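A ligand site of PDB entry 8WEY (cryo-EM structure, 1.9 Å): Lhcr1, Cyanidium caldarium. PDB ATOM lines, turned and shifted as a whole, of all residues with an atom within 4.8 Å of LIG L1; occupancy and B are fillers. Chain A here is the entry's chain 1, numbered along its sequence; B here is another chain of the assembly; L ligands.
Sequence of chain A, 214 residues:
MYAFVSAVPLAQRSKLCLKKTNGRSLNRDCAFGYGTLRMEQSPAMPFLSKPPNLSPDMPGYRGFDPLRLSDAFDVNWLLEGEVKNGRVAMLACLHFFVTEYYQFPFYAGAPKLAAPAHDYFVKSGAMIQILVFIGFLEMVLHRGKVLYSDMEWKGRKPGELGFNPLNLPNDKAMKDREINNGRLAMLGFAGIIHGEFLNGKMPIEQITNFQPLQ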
ATOM      1  N   PRO A  43     -15.886  -9.299 -29.977  1.00  0.00           N
ATOM      2  CA  PRO A  43     -14.794  -8.846 -30.856  1.00  0.00           C
ATOM      3  C   PRO A  43     -14.329  -7.402 -30.611  1.00  0.00           C
ATOM      4  O   PRO A  43     -13.135  -7.178 -30.595  1.00  0.00           O
ATOM      5  CB  PRO A  43     -15.382  -8.975 -32.276  1.00  0.00           C
ATOM      6  CG  PRO A  43     -16.448 -10.034 -32.131  1.00  0.00           C
ATOM      7  CD  PRO A  43     -17.009  -9.864 -30.740  1.00  0.00           C
ATOM      8  N   ALA A  44     -15.267  -6.467 -30.441  1.00  0.00           N
ATOM      9  CA  ALA A  44     -15.002  -5.021 -30.251  1.00  0.00           C
ATOM     10  C   ALA A  44     -14.399  -4.754 -28.866  1.00  0.00           C
ATOM     11  O   ALA A  44     -13.573  -3.826 -28.767  1.00  0.00           O
ATOM     12  CB  ALA A  44     -16.264  -4.217 -30.452  1.00  0.00           C
ATOM     13  N   MET A  45     -14.815  -5.506 -27.835  1.00  0.00           N
ATOM     14  CA  MET A  45     -14.405  -5.326 -26.418  1.00  0.00           C
ATOM     15  C   MET A  45     -14.123  -6.691 -25.800  1.00  0.00           C
ATOM     16  O   MET A  45     -14.936  -7.204 -25.022  1.00  0.00           O
ATOM     17  CB  MET A  45     -15.509  -4.594 -25.638  1.00  0.00           C
ATOM     18  CG  MET A  45     -15.764  -3.182 -26.146  1.00  0.00           C
ATOM     19  SD  MET A  45     -17.228  -2.401 -25.409  1.00  0.00           S
ATOM     20  CE  MET A  45     -16.518  -1.696 -23.925  1.00  0.00           C
ATOM     21  N   PRO A  46     -12.967  -7.325 -26.131  1.00  0.00           N
ATOM     22  CA  PRO A  46     -12.676  -8.705 -25.731  1.00  0.00           C
ATOM     23  C   PRO A  46     -12.808  -9.029 -24.234  1.00  0.00           C
ATOM     24  O   PRO A  46     -13.152 -10.147 -23.896  1.00  0.00           O
ATOM     25  CB  PRO A  46     -11.205  -8.897 -26.151  1.00  0.00           C
ATOM     26  CG  PRO A  46     -11.030  -7.928 -27.298  1.00  0.00           C
ATOM     27  CD  PRO A  46     -11.872  -6.738 -26.917  1.00  0.00           C
ATOM     28  N   PHE A  47     -12.494  -8.043 -23.390  1.00  0.00           N
ATOM     29  CA  PHE A  47     -12.631  -8.075 -21.904  1.00  0.00           C
ATOM     30  C   PHE A  47     -14.091  -8.283 -21.475  1.00  0.00           C
ATOM     31  O   PHE A  47     -14.293  -8.901 -20.410  1.00  0.00           O
ATOM     32  CB  PHE A  47     -12.035  -6.815 -21.279  1.00  0.00           C
ATOM     33  CG  PHE A  47     -12.580  -5.509 -21.786  1.00  0.00           C
ATOM     34  CD1 PHE A  47     -12.033  -4.893 -22.909  1.00  0.00           C
ATOM     35  CD2 PHE A  47     -13.619  -4.867 -21.131  1.00  0.00           C
ATOM     36  CE1 PHE A  47     -12.529  -3.688 -23.372  1.00  0.00           C
ATOM     37  CE2 PHE A  47     -14.114  -3.648 -21.598  1.00  0.00           C
ATOM     38  CZ  PHE A  47     -13.569  -3.071 -22.721  1.00  0.00           C
ATOM     39  N   ARG A  62     -19.951  -5.917 -34.597  1.00  0.00           N
ATOM     40  CA  ARG A  62     -18.636  -5.995 -33.911  1.00  0.00           C
ATOM     41  C   ARG A  62     -18.805  -6.631 -32.523  1.00  0.00           C
ATOM     42  O   ARG A  62     -17.805  -6.702 -31.784  1.00  0.00           O
ATOM     43  CB  ARG A  62     -18.017  -4.598 -33.778  1.00  0.00           C
ATOM     44  CG  ARG A  62     -18.213  -3.686 -34.972  1.00  0.00           C
ATOM     45  CD  ARG A  62     -17.521  -4.171 -36.226  1.00  0.00           C
ATOM     46  NE  ARG A  62     -17.327  -3.069 -37.157  1.00  0.00           N
ATOM     47  CZ  ARG A  62     -17.114  -3.184 -38.475  1.00  0.00           C
ATOM     48  NH1 ARG A  62     -17.054  -4.367 -39.062  1.00  0.00           N
ATOM     49  NH2 ARG A  62     -16.942  -2.093 -39.202  1.00  0.00           N
ATOM     50  N   PHE A  64     -20.558  -5.100 -30.293  1.00  0.00           N
ATOM     51  CA  PHE A  64     -20.453  -3.864 -29.472  1.00  0.00           C
ATOM     52  C   PHE A  64     -21.810  -3.532 -28.857  1.00  0.00           C
ATOM     53  O   PHE A  64     -22.665  -2.938 -29.547  1.00  0.00           O
ATOM     54  CB  PHE A  64     -19.918  -2.691 -30.306  1.00  0.00           C
ATOM     55  CG  PHE A  64     -19.814  -1.405 -29.535  1.00  0.00           C
ATOM     56  CD1 PHE A  64     -18.960  -1.289 -28.452  1.00  0.00           C
ATOM     57  CD2 PHE A  64     -20.588  -0.300 -29.880  1.00  0.00           C
ATOM     58  CE1 PHE A  64     -18.864  -0.101 -27.740  1.00  0.00           C
ATOM     59  CE2 PHE A  64     -20.504   0.884 -29.162  1.00  0.00           C
ATOM     60  CZ  PHE A  64     -19.640   0.981 -28.089  1.00  0.00           C
ATOM     61  N   TRP B 139     -15.859   6.528 -20.126  1.00  0.00           N
ATOM     62  CA  TRP B 139     -15.079   5.272 -19.955  1.00  0.00           C
ATOM     63  C   TRP B 139     -15.639   4.486 -18.766  1.00  0.00           C
ATOM     64  O   TRP B 139     -15.999   3.321 -18.953  1.00  0.00           O
ATOM     65  CB  TRP B 139     -13.578   5.543 -19.790  1.00  0.00           C
ATOM     66  CG  TRP B 139     -12.784   4.286 -19.539  1.00  0.00           C
ATOM     67  CD1 TRP B 139     -12.600   3.656 -18.345  1.00  0.00           C
ATOM     68  CD2 TRP B 139     -12.090   3.496 -20.519  1.00  0.00           C
ATOM     69  NE1 TRP B 139     -11.846   2.532 -18.513  1.00  0.00           N
ATOM     70  CE2 TRP B 139     -11.518   2.404 -19.840  1.00  0.00           C
ATOM     71  CE3 TRP B 139     -11.894   3.616 -21.901  1.00  0.00           C
ATOM     72  CZ2 TRP B 139     -10.759   1.429 -20.494  1.00  0.00           C
ATOM     73  CZ3 TRP B 139     -11.135   2.651 -22.546  1.00  0.00           C
ATOM     74  CH2 TRP B 139     -10.580   1.583 -21.850  1.00  0.00           C
ATOM     75  N   PHE B 142     -19.395   3.263 -19.409  1.00  0.00           N
ATOM     76  CA  PHE B 142     -19.591   2.399 -20.607  1.00  0.00           C
ATOM     77  C   PHE B 142     -18.528   1.296 -20.695  1.00  0.00           C
ATOM     78  O   PHE B 142     -18.722   0.394 -21.533  1.00  0.00           O
ATOM     79  CB  PHE B 142     -19.585   3.232 -21.887  1.00  0.00           C
ATOM     80  CG  PHE B 142     -20.725   4.210 -22.024  1.00  0.00           C
ATOM     81  CD1 PHE B 142     -22.048   3.775 -22.024  1.00  0.00           C
ATOM     82  CD2 PHE B 142     -20.487   5.560 -22.195  1.00  0.00           C
ATOM     83  CE1 PHE B 142     -23.094   4.667 -22.169  1.00  0.00           C
ATOM     84  CE2 PHE B 142     -21.538   6.468 -22.338  1.00  0.00           C
ATOM     85  CZ  PHE B 142     -22.839   6.013 -22.326  1.00  0.00           C
ATOM     86  N   VAL B 143     -17.448   1.358 -19.908  1.00  0.00           N
ATOM     87  CA  VAL B 143     -16.308   0.385 -19.979  1.00  0.00           C
ATOM     88  C   VAL B 143     -15.947  -0.094 -18.569  1.00  0.00           C
ATOM     89  O   VAL B 143     -16.037  -1.317 -18.332  1.00  0.00           O
ATOM     90  CB  VAL B 143     -15.071   0.986 -20.696  1.00  0.00           C
ATOM     91  CG1 VAL B 143     -14.105  -0.099 -21.117  1.00  0.00           C
ATOM     92  CG2 VAL B 143     -15.451   1.837 -21.889  1.00  0.00           C
ATOM     93  N   PHE B 161      -8.117  -5.268 -19.828  1.00  0.00           N
ATOM     94  CA  PHE B 161      -8.882  -4.738 -20.989  1.00  0.00           C
ATOM     95  C   PHE B 161      -8.295  -5.296 -22.297  1.00  0.00           C
ATOM     96  O   PHE B 161      -8.685  -4.811 -23.377  1.00  0.00           O
ATOM     97  CB  PHE B 161      -8.915  -3.212 -20.970  1.00  0.00           C
ATOM     98  CG  PHE B 161      -9.632  -2.628 -19.780  1.00  0.00           C
ATOM     99  CD1 PHE B 161     -11.007  -2.476 -19.784  1.00  0.00           C
ATOM    100  CD2 PHE B 161      -8.933  -2.230 -18.648  1.00  0.00           C
ATOM    101  CE1 PHE B 161     -11.677  -1.949 -18.694  1.00  0.00           C
ATOM    102  CE2 PHE B 161      -9.602  -1.692 -17.549  1.00  0.00           C
ATOM    103  CZ  PHE B 161     -10.971  -1.552 -17.582  1.00  0.00           C
ATOM    104  N   GLY B 162      -7.409  -6.295 -22.208  1.00  0.00           N
ATOM    105  CA  GLY B 162      -6.721  -6.932 -23.343  1.00  0.00           C
ATOM    106  C   GLY B 162      -6.040  -5.933 -24.268  1.00  0.00           C
ATOM    107  O   GLY B 162      -5.925  -6.240 -25.472  1.00  0.00           O
ATOM    108  N   PHE B 163      -5.579  -4.794 -23.727  1.00  0.00           N
ATOM    109  CA  PHE B 163      -4.919  -3.698 -24.480  1.00  0.00           C
ATOM    110  C   PHE B 163      -3.399  -3.950 -24.490  1.00  0.00           C
ATOM    111  O   PHE B 163      -2.736  -3.682 -23.467  1.00  0.00           O
ATOM    112  CB  PHE B 163      -5.224  -2.325 -23.864  1.00  0.00           C
ATOM    113  CG  PHE B 163      -4.531  -1.170 -24.533  1.00  0.00           C
ATOM    114  CD1 PHE B 163      -4.971  -0.703 -25.770  1.00  0.00           C
ATOM    115  CD2 PHE B 163      -3.436  -0.558 -23.951  1.00  0.00           C
ATOM    116  CE1 PHE B 163      -4.326   0.352 -26.394  1.00  0.00           C
ATOM    117  CE2 PHE B 163      -2.797   0.503 -24.582  1.00  0.00           C
ATOM    118  CZ  PHE B 163      -3.245   0.958 -25.792  1.00  0.00           C
HETATM  119 MG1  LIG L   1     -12.494  -2.038 -29.347  1.00  0.00          MG
HETATM  120  C1  LIG L   1     -13.027  -2.767 -32.696  1.00  0.00           C
HETATM  121  C2  LIG L   1      -9.660  -3.919 -29.501  1.00  0.00           C
HETATM  122  C3  LIG L   1     -11.780  -0.910 -26.246  1.00  0.00           C
HETATM  123  C4  LIG L   1     -15.362   0.272 -29.508  1.00  0.00           C
HETATM  124  N1  LIG L   1     -11.489  -3.116 -30.820  1.00  0.00           N
HETATM  125  C5  LIG L   1     -11.828  -3.369 -32.037  1.00  0.00           C
HETATM  126  C6  LIG L   1     -10.958  -4.331 -32.810  1.00  0.00           C
HETATM  127  C7  LIG L   1      -9.900  -4.707 -31.765  1.00  0.00           C
HETATM  128  C8  LIG L   1     -10.391  -3.854 -30.619  1.00  0.00           C
HETATM  129  C9  LIG L   1      -9.901  -6.192 -31.421  1.00  0.00           C
HETATM  130  C10 LIG L   1     -10.266  -3.717 -34.047  1.00  0.00           C
HETATM  131  C11 LIG L   1      -9.578  -2.354 -33.830  1.00  0.00           C
HETATM  132  C12 LIG L   1     -10.378  -1.216 -34.415  1.00  0.00           C
HETATM  133  O1  LIG L   1     -11.032  -0.468 -33.698  1.00  0.00           O
HETATM  134  O2  LIG L   1     -10.364  -0.980 -35.847  1.00  0.00           O
HETATM  135  N2  LIG L   1     -10.948  -2.375 -28.057  1.00  0.00           N
HETATM  136  C13 LIG L   1      -9.903  -3.183 -28.250  1.00  0.00           C
HETATM  137  C14 LIG L   1      -8.953  -3.256 -27.127  1.00  0.00           C
HETATM  138  C15 LIG L   1      -9.578  -2.356 -26.126  1.00  0.00           C
HETATM  139  C16 LIG L   1     -10.809  -1.861 -26.833  1.00  0.00           C
HETATM  140  C17 LIG L   1      -7.686  -4.049 -26.996  1.00  0.00           C
HETATM  141  C18 LIG L   1      -8.977  -2.065 -24.793  1.00  0.00           C
HETATM  142  C19 LIG L   1      -9.364  -1.162 -23.913  1.00  0.00           C
HETATM  143  N3  LIG L   1     -13.393  -0.608 -28.163  1.00  0.00           N
HETATM  144  C20 LIG L   1     -12.956  -0.336 -26.916  1.00  0.00           C
HETATM  145  C21 LIG L   1     -13.758   0.682 -26.180  1.00  0.00           C
HETATM  146  C22 LIG L   1     -14.828   1.035 -27.129  1.00  0.00           C
HETATM  147  C23 LIG L   1     -14.498   0.175 -28.308  1.00  0.00           C
HETATM  148  C24 LIG L   1     -13.562   1.219 -24.783  1.00  0.00           C
HETATM  149  C25 LIG L   1     -15.956   2.035 -26.925  1.00  0.00           C
HETATM  150  C26 LIG L   1     -16.679   1.744 -25.624  1.00  0.00           C
HETATM  151  N4  LIG L   1     -13.842  -1.331 -30.681  1.00  0.00           N
HETATM  152  C27 LIG L   1     -14.996  -0.483 -30.703  1.00  0.00           C
HETATM  153  C28 LIG L   1     -15.749  -0.445 -31.978  1.00  0.00           C
HETATM  154  C29 LIG L   1     -14.927  -1.386 -32.787  1.00  0.00           C
HETATM  155  C30 LIG L   1     -13.890  -1.827 -31.976  1.00  0.00           C
HETATM  156  C31 LIG L   1     -16.979   0.272 -32.442  1.00  0.00           C
HETATM  157  C32 LIG L   1     -14.769  -2.052 -34.111  1.00  0.00           C
HETATM  158  O3  LIG L   1     -15.541  -1.898 -35.124  1.00  0.00           O
HETATM  159  C33 LIG L   1     -13.572  -2.927 -34.068  1.00  0.00           C
HETATM  160  C34 LIG L   1     -13.974  -4.342 -34.384  1.00  0.00           C
HETATM  161  O4  LIG L   1     -14.377  -5.107 -33.526  1.00  0.00           O
HETATM  162  O5  LIG L   1     -13.901  -4.814 -35.753  1.00  0.00           O
HETATM  163  C35 LIG L   1     -13.334  -6.097 -36.059  1.00  0.00           C
HETATM  164  C1  LG2 L   2     -17.322  10.743 -32.098  1.00  0.00           C
HETATM  165  C2  LG2 L   2     -17.565  11.398 -30.703  1.00  0.00           C
HETATM  166  C3  LG2 L   2     -16.417   9.512 -31.959  1.00  0.00           C
HETATM  167  C4  LG2 L   2     -18.966  19.202 -24.659  1.00  0.00           C
HETATM  168  C5  LG2 L   2     -18.211  12.805 -30.626  1.00  0.00           C
HETATM  169  C6  LG2 L   2     -19.197   5.079 -38.097  1.00  0.00           C
HETATM  170  C7  LG2 L   2     -16.675   5.266 -36.404  1.00  0.00           C
HETATM  171  C8  LG2 L   2     -17.115   6.146 -35.215  1.00  0.00           C
HETATM  172  C9  LG2 L   2     -16.750   7.660 -35.288  1.00  0.00           C
HETATM  173  C10 LG2 L   2     -17.466  13.693 -29.592  1.00  0.00           C
HETATM  174  C11 LG2 L   2     -15.987   8.153 -34.050  1.00  0.00           C
HETATM  175  C12 LG2 L   2     -16.893   8.321 -32.817  1.00  0.00           C
HETATM  176  C13 LG2 L   2     -16.294  23.458 -22.724  1.00  0.00           C
HETATM  177  C14 LG2 L   2     -16.585  23.779 -24.197  1.00  0.00           C
HETATM  178  C15 LG2 L   2     -16.904  25.332 -24.328  1.00  0.00           C
HETATM  179  C16 LG2 L   2     -19.029  14.812 -26.927  1.00  0.00           C
HETATM  180  C17 LG2 L   2     -18.252  25.783 -23.636  1.00  0.00           C
HETATM  181  C18 LG2 L   2     -19.342  24.692 -23.620  1.00  0.00           C
HETATM  182  C19 LG2 L   2     -19.133  23.557 -24.570  1.00  0.00           C
HETATM  183  C20 LG2 L   2     -17.785  22.992 -24.720  1.00  0.00           C
HETATM  184  C21 LG2 L   2     -20.192  19.427 -23.781  1.00  0.00           C
HETATM  185  C22 LG2 L   2     -17.746  21.472 -24.300  1.00  0.00           C
HETATM  186  C23 LG2 L   2     -18.415  20.508 -25.320  1.00  0.00           C
HETATM  187  C24 LG2 L   2     -18.190  15.019 -29.325  1.00  0.00           C
HETATM  188  C25 LG2 L   2     -15.366  23.453 -25.063  1.00  0.00           C
HETATM  189  C26 LG2 L   2     -18.031  15.494 -27.862  1.00  0.00           C
HETATM  190  C27 LG2 L   2     -17.986  17.043 -27.748  1.00  0.00           C
HETATM  191  C28 LG2 L   2     -17.788  17.568 -26.303  1.00  0.00           C
HETATM  192  C29 LG2 L   2     -19.119  17.997 -25.628  1.00  0.00           C
HETATM  193  C30 LG2 L   2     -19.693  23.907 -25.962  1.00  0.00           C
HETATM  194  C31 LG2 L   2     -16.613   2.909 -34.488  1.00  0.00           C
HETATM  195  C32 LG2 L   2     -16.946   2.801 -35.982  1.00  0.00           C
HETATM  196  C33 LG2 L   2     -17.564   4.008 -36.545  1.00  0.00           C
HETATM  197  C34 LG2 L   2     -18.209   3.916 -37.920  1.00  0.00           C
HETATM  198  C35 LG2 L   2     -19.001   2.562 -38.034  1.00  0.00           C
HETATM  199  C36 LG2 L   2     -18.138   1.305 -37.672  1.00  0.00           C
HETATM  200  C37 LG2 L   2     -17.537   1.451 -36.263  1.00  0.00           C
HETATM  201  O1  LG2 L   2     -18.932   0.181 -37.700  1.00  0.00           O
HETATM  202  C38 LG2 L   2     -17.142   3.943 -39.026  1.00  0.00           C
HETATM  203  O2  LG2 L   2     -17.974  26.158 -22.333  1.00  0.00           O
HETATM  204  C39 LG2 L   2     -16.866  11.668 -33.242  1.00  0.00           C
HETATM  205  C40 LG2 L   2     -16.108   8.157 -36.582  1.00  0.00           C
HETATM  206 MG1  LG3 L   3     -25.392   0.888 -33.338  1.00  0.00          MG
HETATM  207  C1  LG3 L   3     -24.457  -2.383 -32.734  1.00  0.00           C
HETATM  208  C2  LG3 L   3     -28.549   0.055 -32.491  1.00  0.00           C
HETATM  209  C3  LG3 L   3     -26.145   4.208 -33.501  1.00  0.00           C
HETATM  210  C4  LG3 L   3     -21.854   1.697 -33.851  1.00  0.00           C
HETATM  211  N1  LG3 L   3     -26.333  -0.833 -32.674  1.00  0.00           N
HETATM  212  C5  LG3 L   3     -25.887  -2.017 -32.563  1.00  0.00           C
HETATM  213  C6  LG3 L   3     -26.867  -3.077 -32.183  1.00  0.00           C
HETATM  214  C7  LG3 L   3     -28.170  -2.305 -32.198  1.00  0.00           C
HETATM  215  C8  LG3 L   3     -27.647  -0.930 -32.463  1.00  0.00           C
HETATM  216  C9  LG3 L   3     -29.017  -2.795 -33.383  1.00  0.00           C
HETATM  217  C10 LG3 L   3     -26.606  -3.582 -30.762  1.00  0.00           C
HETATM  218  C11 LG3 L   3     -26.185  -2.507 -29.761  1.00  0.00           C
HETATM  219  C12 LG3 L   3     -27.368  -1.794 -29.147  1.00  0.00           C
HETATM  220  O1  LG3 L   3     -28.236  -2.430 -28.563  1.00  0.00           O
HETATM  221  O2  LG3 L   3     -27.457  -0.360 -29.282  1.00  0.00           O
HETATM  222  N2  LG3 L   3     -27.090   1.967 -33.006  1.00  0.00           N
HETATM  223  C13 LG3 L   3     -28.295   1.479 -32.764  1.00  0.00           C
HETATM  224  C14 LG3 L   3     -29.387   2.486 -32.793  1.00  0.00           C
HETATM  225  C15 LG3 L   3     -28.649   3.738 -33.100  1.00  0.00           C
HETATM  226  C16 LG3 L   3     -27.245   3.286 -33.200  1.00  0.00           C
HETATM  227  C17 LG3 L   3     -30.852   2.289 -32.578  1.00  0.00           C
HETATM  228  C18 LG3 L   3     -29.101   5.147 -33.276  1.00  0.00           C
HETATM  229  C19 LG3 L   3     -30.358   5.545 -33.169  1.00  0.00           C
HETATM  230  N3  LG3 L   3     -24.222   2.580 -33.556  1.00  0.00           N
HETATM  231  C20 LG3 L   3     -24.739   3.823 -33.683  1.00  0.00           C
HETATM  232  C21 LG3 L   3     -23.765   4.876 -34.065  1.00  0.00           C
HETATM  233  C22 LG3 L   3     -22.512   4.119 -34.180  1.00  0.00           C
HETATM  234  C23 LG3 L   3     -22.906   2.741 -33.836  1.00  0.00           C
HETATM  235  C24 LG3 L   3     -23.978   6.355 -34.308  1.00  0.00           C
HETATM  236  C25 LG3 L   3     -21.137   4.637 -34.528  1.00  0.00           C
HETATM  237  C26 LG3 L   3     -20.390   4.727 -33.219  1.00  0.00           C
HETATM  238  N4  LG3 L   3     -23.577  -0.004 -33.275  1.00  0.00           N
HETATM  239  C27 LG3 L   3     -22.217   0.319 -33.563  1.00  0.00           C
HETATM  240  C28 LG3 L   3     -21.276  -0.823 -33.557  1.00  0.00           C
HETATM  241  C29 LG3 L   3     -22.216  -1.932 -33.219  1.00  0.00           C
HETATM  242  C30 LG3 L   3     -23.465  -1.357 -33.061  1.00  0.00           C
HETATM  243  C31 LG3 L   3     -19.812  -0.955 -33.803  1.00  0.00           C
HETATM  244  C32 LG3 L   3     -22.344  -3.388 -32.964  1.00  0.00           C
HETATM  245  O3  LG3 L   3     -21.385  -4.239 -32.990  1.00  0.00           O
HETATM  246  C33 LG3 L   3     -23.758  -3.701 -32.642  1.00  0.00           C
HETATM  247  C34 LG3 L   3     -24.249  -4.741 -33.606  1.00  0.00           C
HETATM  248  O4  LG3 L   3     -23.999  -5.920 -33.384  1.00  0.00           O
HETATM  249  O5  LG3 L   3     -25.022  -4.369 -34.786  1.00  0.00           O
HETATM  250  C35 LG3 L   3     -25.280  -5.277 -35.850  1.00  0.00           C
HETATM  251  C36 LG3 L   3     -28.674   0.340 -29.031  1.00  0.00           C
HETATM  252  C37 LG3 L   3     -28.341   1.807 -28.891  1.00  0.00           C
HETATM  253  C38 LG3 L   3     -29.289   2.736 -28.658  1.00  0.00           C
HETATM  254  C39 LG3 L   3     -30.756   2.427 -28.518  1.00  0.00           C
HETATM  255  C40 LG3 L   3     -28.858   4.180 -28.523  1.00  0.00           C
HETATM  256  C41 LG3 L   3     -28.856   4.626 -27.067  1.00  0.00           C
HETATM  257  C42 LG3 L   3     -27.772   5.655 -26.828  1.00  0.00           C
HETATM  258  C43 LG3 L   3     -27.866   6.354 -25.467  1.00  0.00           C
HETATM  259  C44 LG3 L   3     -29.119   7.223 -25.335  1.00  0.00           C
HETATM  260  C45 LG3 L   3     -26.583   7.150 -25.182  1.00  0.00           C
HETATM  261  C46 LG3 L   3     -26.229   8.213 -26.224  1.00  0.00           C
HETATM  262  C47 LG3 L   3     -24.988   9.002 -25.806  1.00  0.00           C
HETATM  263  C48 LG3 L   3     -23.708   8.227 -26.123  1.00  0.00           C
HETATM  264  C49 LG3 L   3     -22.484   8.911 -25.508  1.00  0.00           C
HETATM  265  C1  LG4 L   4     -23.156  11.958 -29.267  1.00  0.00           C
HETATM  266  C2  LG4 L   4     -24.031  12.662 -30.350  1.00  0.00           C
HETATM  267  C3  LG4 L   4     -22.089  11.040 -29.885  1.00  0.00           C
HETATM  268  C4  LG4 L   4     -30.428  18.717 -32.886  1.00  0.00           C
HETATM  269  C5  LG4 L   4     -25.473  12.979 -29.893  1.00  0.00           C
HETATM  270  C6  LG4 L   4     -18.107   4.085 -28.883  1.00  0.00           C
HETATM  271  C7  LG4 L   4     -17.936   7.253 -29.493  1.00  0.00           C
HETATM  272  C8  LG4 L   4     -17.748   8.497 -28.595  1.00  0.00           C
HETATM  273  C9  LG4 L   4     -19.077   9.163 -28.133  1.00  0.00           C
HETATM  274  C10 LG4 L   4     -25.905  14.469 -30.034  1.00  0.00           C
HETATM  275  C11 LG4 L   4     -19.977   9.647 -29.302  1.00  0.00           C
HETATM  276  C12 LG4 L   4     -21.387  10.109 -28.857  1.00  0.00           C
HETATM  277  C13 LG4 L   4     -32.882  22.220 -34.753  1.00  0.00           C
HETATM  278  C14 LG4 L   4     -34.020  21.975 -33.758  1.00  0.00           C
HETATM  279  C15 LG4 L   4     -34.718  23.348 -33.382  1.00  0.00           C
HETATM  280  C16 LG4 L   4     -27.835  14.155 -33.439  1.00  0.00           C
HETATM  281  C17 LG4 L   4     -35.640  23.274 -32.109  1.00  0.00           C
HETATM  282  C18 LG4 L   4     -34.832  22.862 -30.869  1.00  0.00           C
HETATM  283  C19 LG4 L   4     -33.728  21.893 -31.135  1.00  0.00           C
HETATM  284  C20 LG4 L   4     -33.506  21.311 -32.484  1.00  0.00           C
HETATM  285  C21 LG4 L   4     -30.726  18.140 -34.266  1.00  0.00           C
HETATM  286  C22 LG4 L   4     -32.784  19.912 -32.583  1.00  0.00           C
HETATM  287  C23 LG4 L   4     -31.231  20.001 -32.487  1.00  0.00           C
HETATM  288  C24 LG4 L   4     -26.279  14.889 -31.482  1.00  0.00           C
HETATM  289  C25 LG4 L   4     -35.093  21.133 -34.440  1.00  0.00           C
HETATM  290  C26 LG4 L   4     -27.709  14.551 -31.969  1.00  0.00           C
HETATM  291  C27 LG4 L   4     -28.833  15.449 -31.415  1.00  0.00           C
HETATM  292  C28 LG4 L   4     -28.827  16.869 -32.027  1.00  0.00           C
HETATM  293  C29 LG4 L   4     -30.125  17.683 -31.770  1.00  0.00           C
HETATM  294  C30 LG4 L   4     -33.493  20.941 -29.959  1.00  0.00           C
HETATM  295  C31 LG4 L   4     -14.666   6.702 -28.310  1.00  0.00           C
HETATM  296  C32 LG4 L   4     -15.494   6.725 -29.599  1.00  0.00           C
HETATM  297  C33 LG4 L   4     -16.826   6.176 -29.324  1.00  0.00           C
HETATM  298  C34 LG4 L   4     -17.207   4.819 -29.880  1.00  0.00           C
HETATM  299  C35 LG4 L   4     -15.906   3.973 -30.121  1.00  0.00           C
HETATM  300  C36 LG4 L   4     -14.881   4.690 -31.076  1.00  0.00           C
HETATM  301  C37 LG4 L   4     -14.662   6.179 -30.724  1.00  0.00           C
HETATM  302  O1  LG4 L   4     -13.673   4.022 -31.007  1.00  0.00           O
HETATM  303  C38 LG4 L   4     -17.935   4.940 -31.211  1.00  0.00           C
HETATM  304  O2  LG4 L   4     -36.217  24.505 -31.884  1.00  0.00           O
HETATM  305  C39 LG4 L   4     -22.531  12.948 -28.267  1.00  0.00           C
HETATM  306  C40 LG4 L   4     -18.826  10.245 -27.070  1.00  0.00           C
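The backbone carbonyl oxygen (O) of Ala 44 is bound to a magnesium atom (MG1) of LIG L1 (2.2 Å).
The backbone NH (N) of Ala 44 sits close to an oxygen (O4) of LIG L1 (3.5 Å).
An oxygen (O3) of LIG L1 lies within hydrogen-bond range of the guanidinium group of Arg 62, at 2.9 Å.
The backbone NH (N) of Arg 62 is in hydrogen-bond range of an oxygen (O3) of LG3 L3 (2.7 Å).
O3 of LG3 L3 lies within hydrogen-bond range of N of Phe 64, at 2.9 Å.
O1 of LG2 L2 sits at hydrogen-bond distance from NH2 of Arg 62 (3.4 Å).
The backbone NH (N) of Ala 44 lies within hydrogen-bond range of the backbone carbonyl oxygen (O) of Arg 62 (2.9 Å).
Pro 43 touches LIG L1.
CE of Met 45 touches C26 of LIG L1, at 3.8 Å.
Phe 64 touches LIG L1 (CE1 to C26, 3.6 Å).
Trp 139 of chain B touches LIG L1.
Val 143 of chain B touches LIG L1 (CG2 to C24, 3.5 Å).
O of Phe 161 of chain B touches C18 of LIG L1, 3.1 Å away.
O of Gly 162 of chain B touches C17 of LIG L1, at 3.2 Å.
CA of Phe 163 of chain B touches C17 of LIG L1 (3.8 Å).
Hydrophobic or aromatic side chains within 4 Å of LIG L1: Ala 44, Met 45, Phe 64, Trp 139 of chain B, Val 143 of chain B, Phe 161 of chain B and Phe 163 of chain B.
Within 4 Å of LIG L1: Pro 43, Ala 44, Met 45, Arg 62, Phe 64, Trp 139 of chain B, Val 143 of chain B, Phe 161 of chain B, Gly 162 of chain B and Phe 163 of chain B.
The nearest printed residue that does not touch LIG L1 is Phe 47 (4.1 Å).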
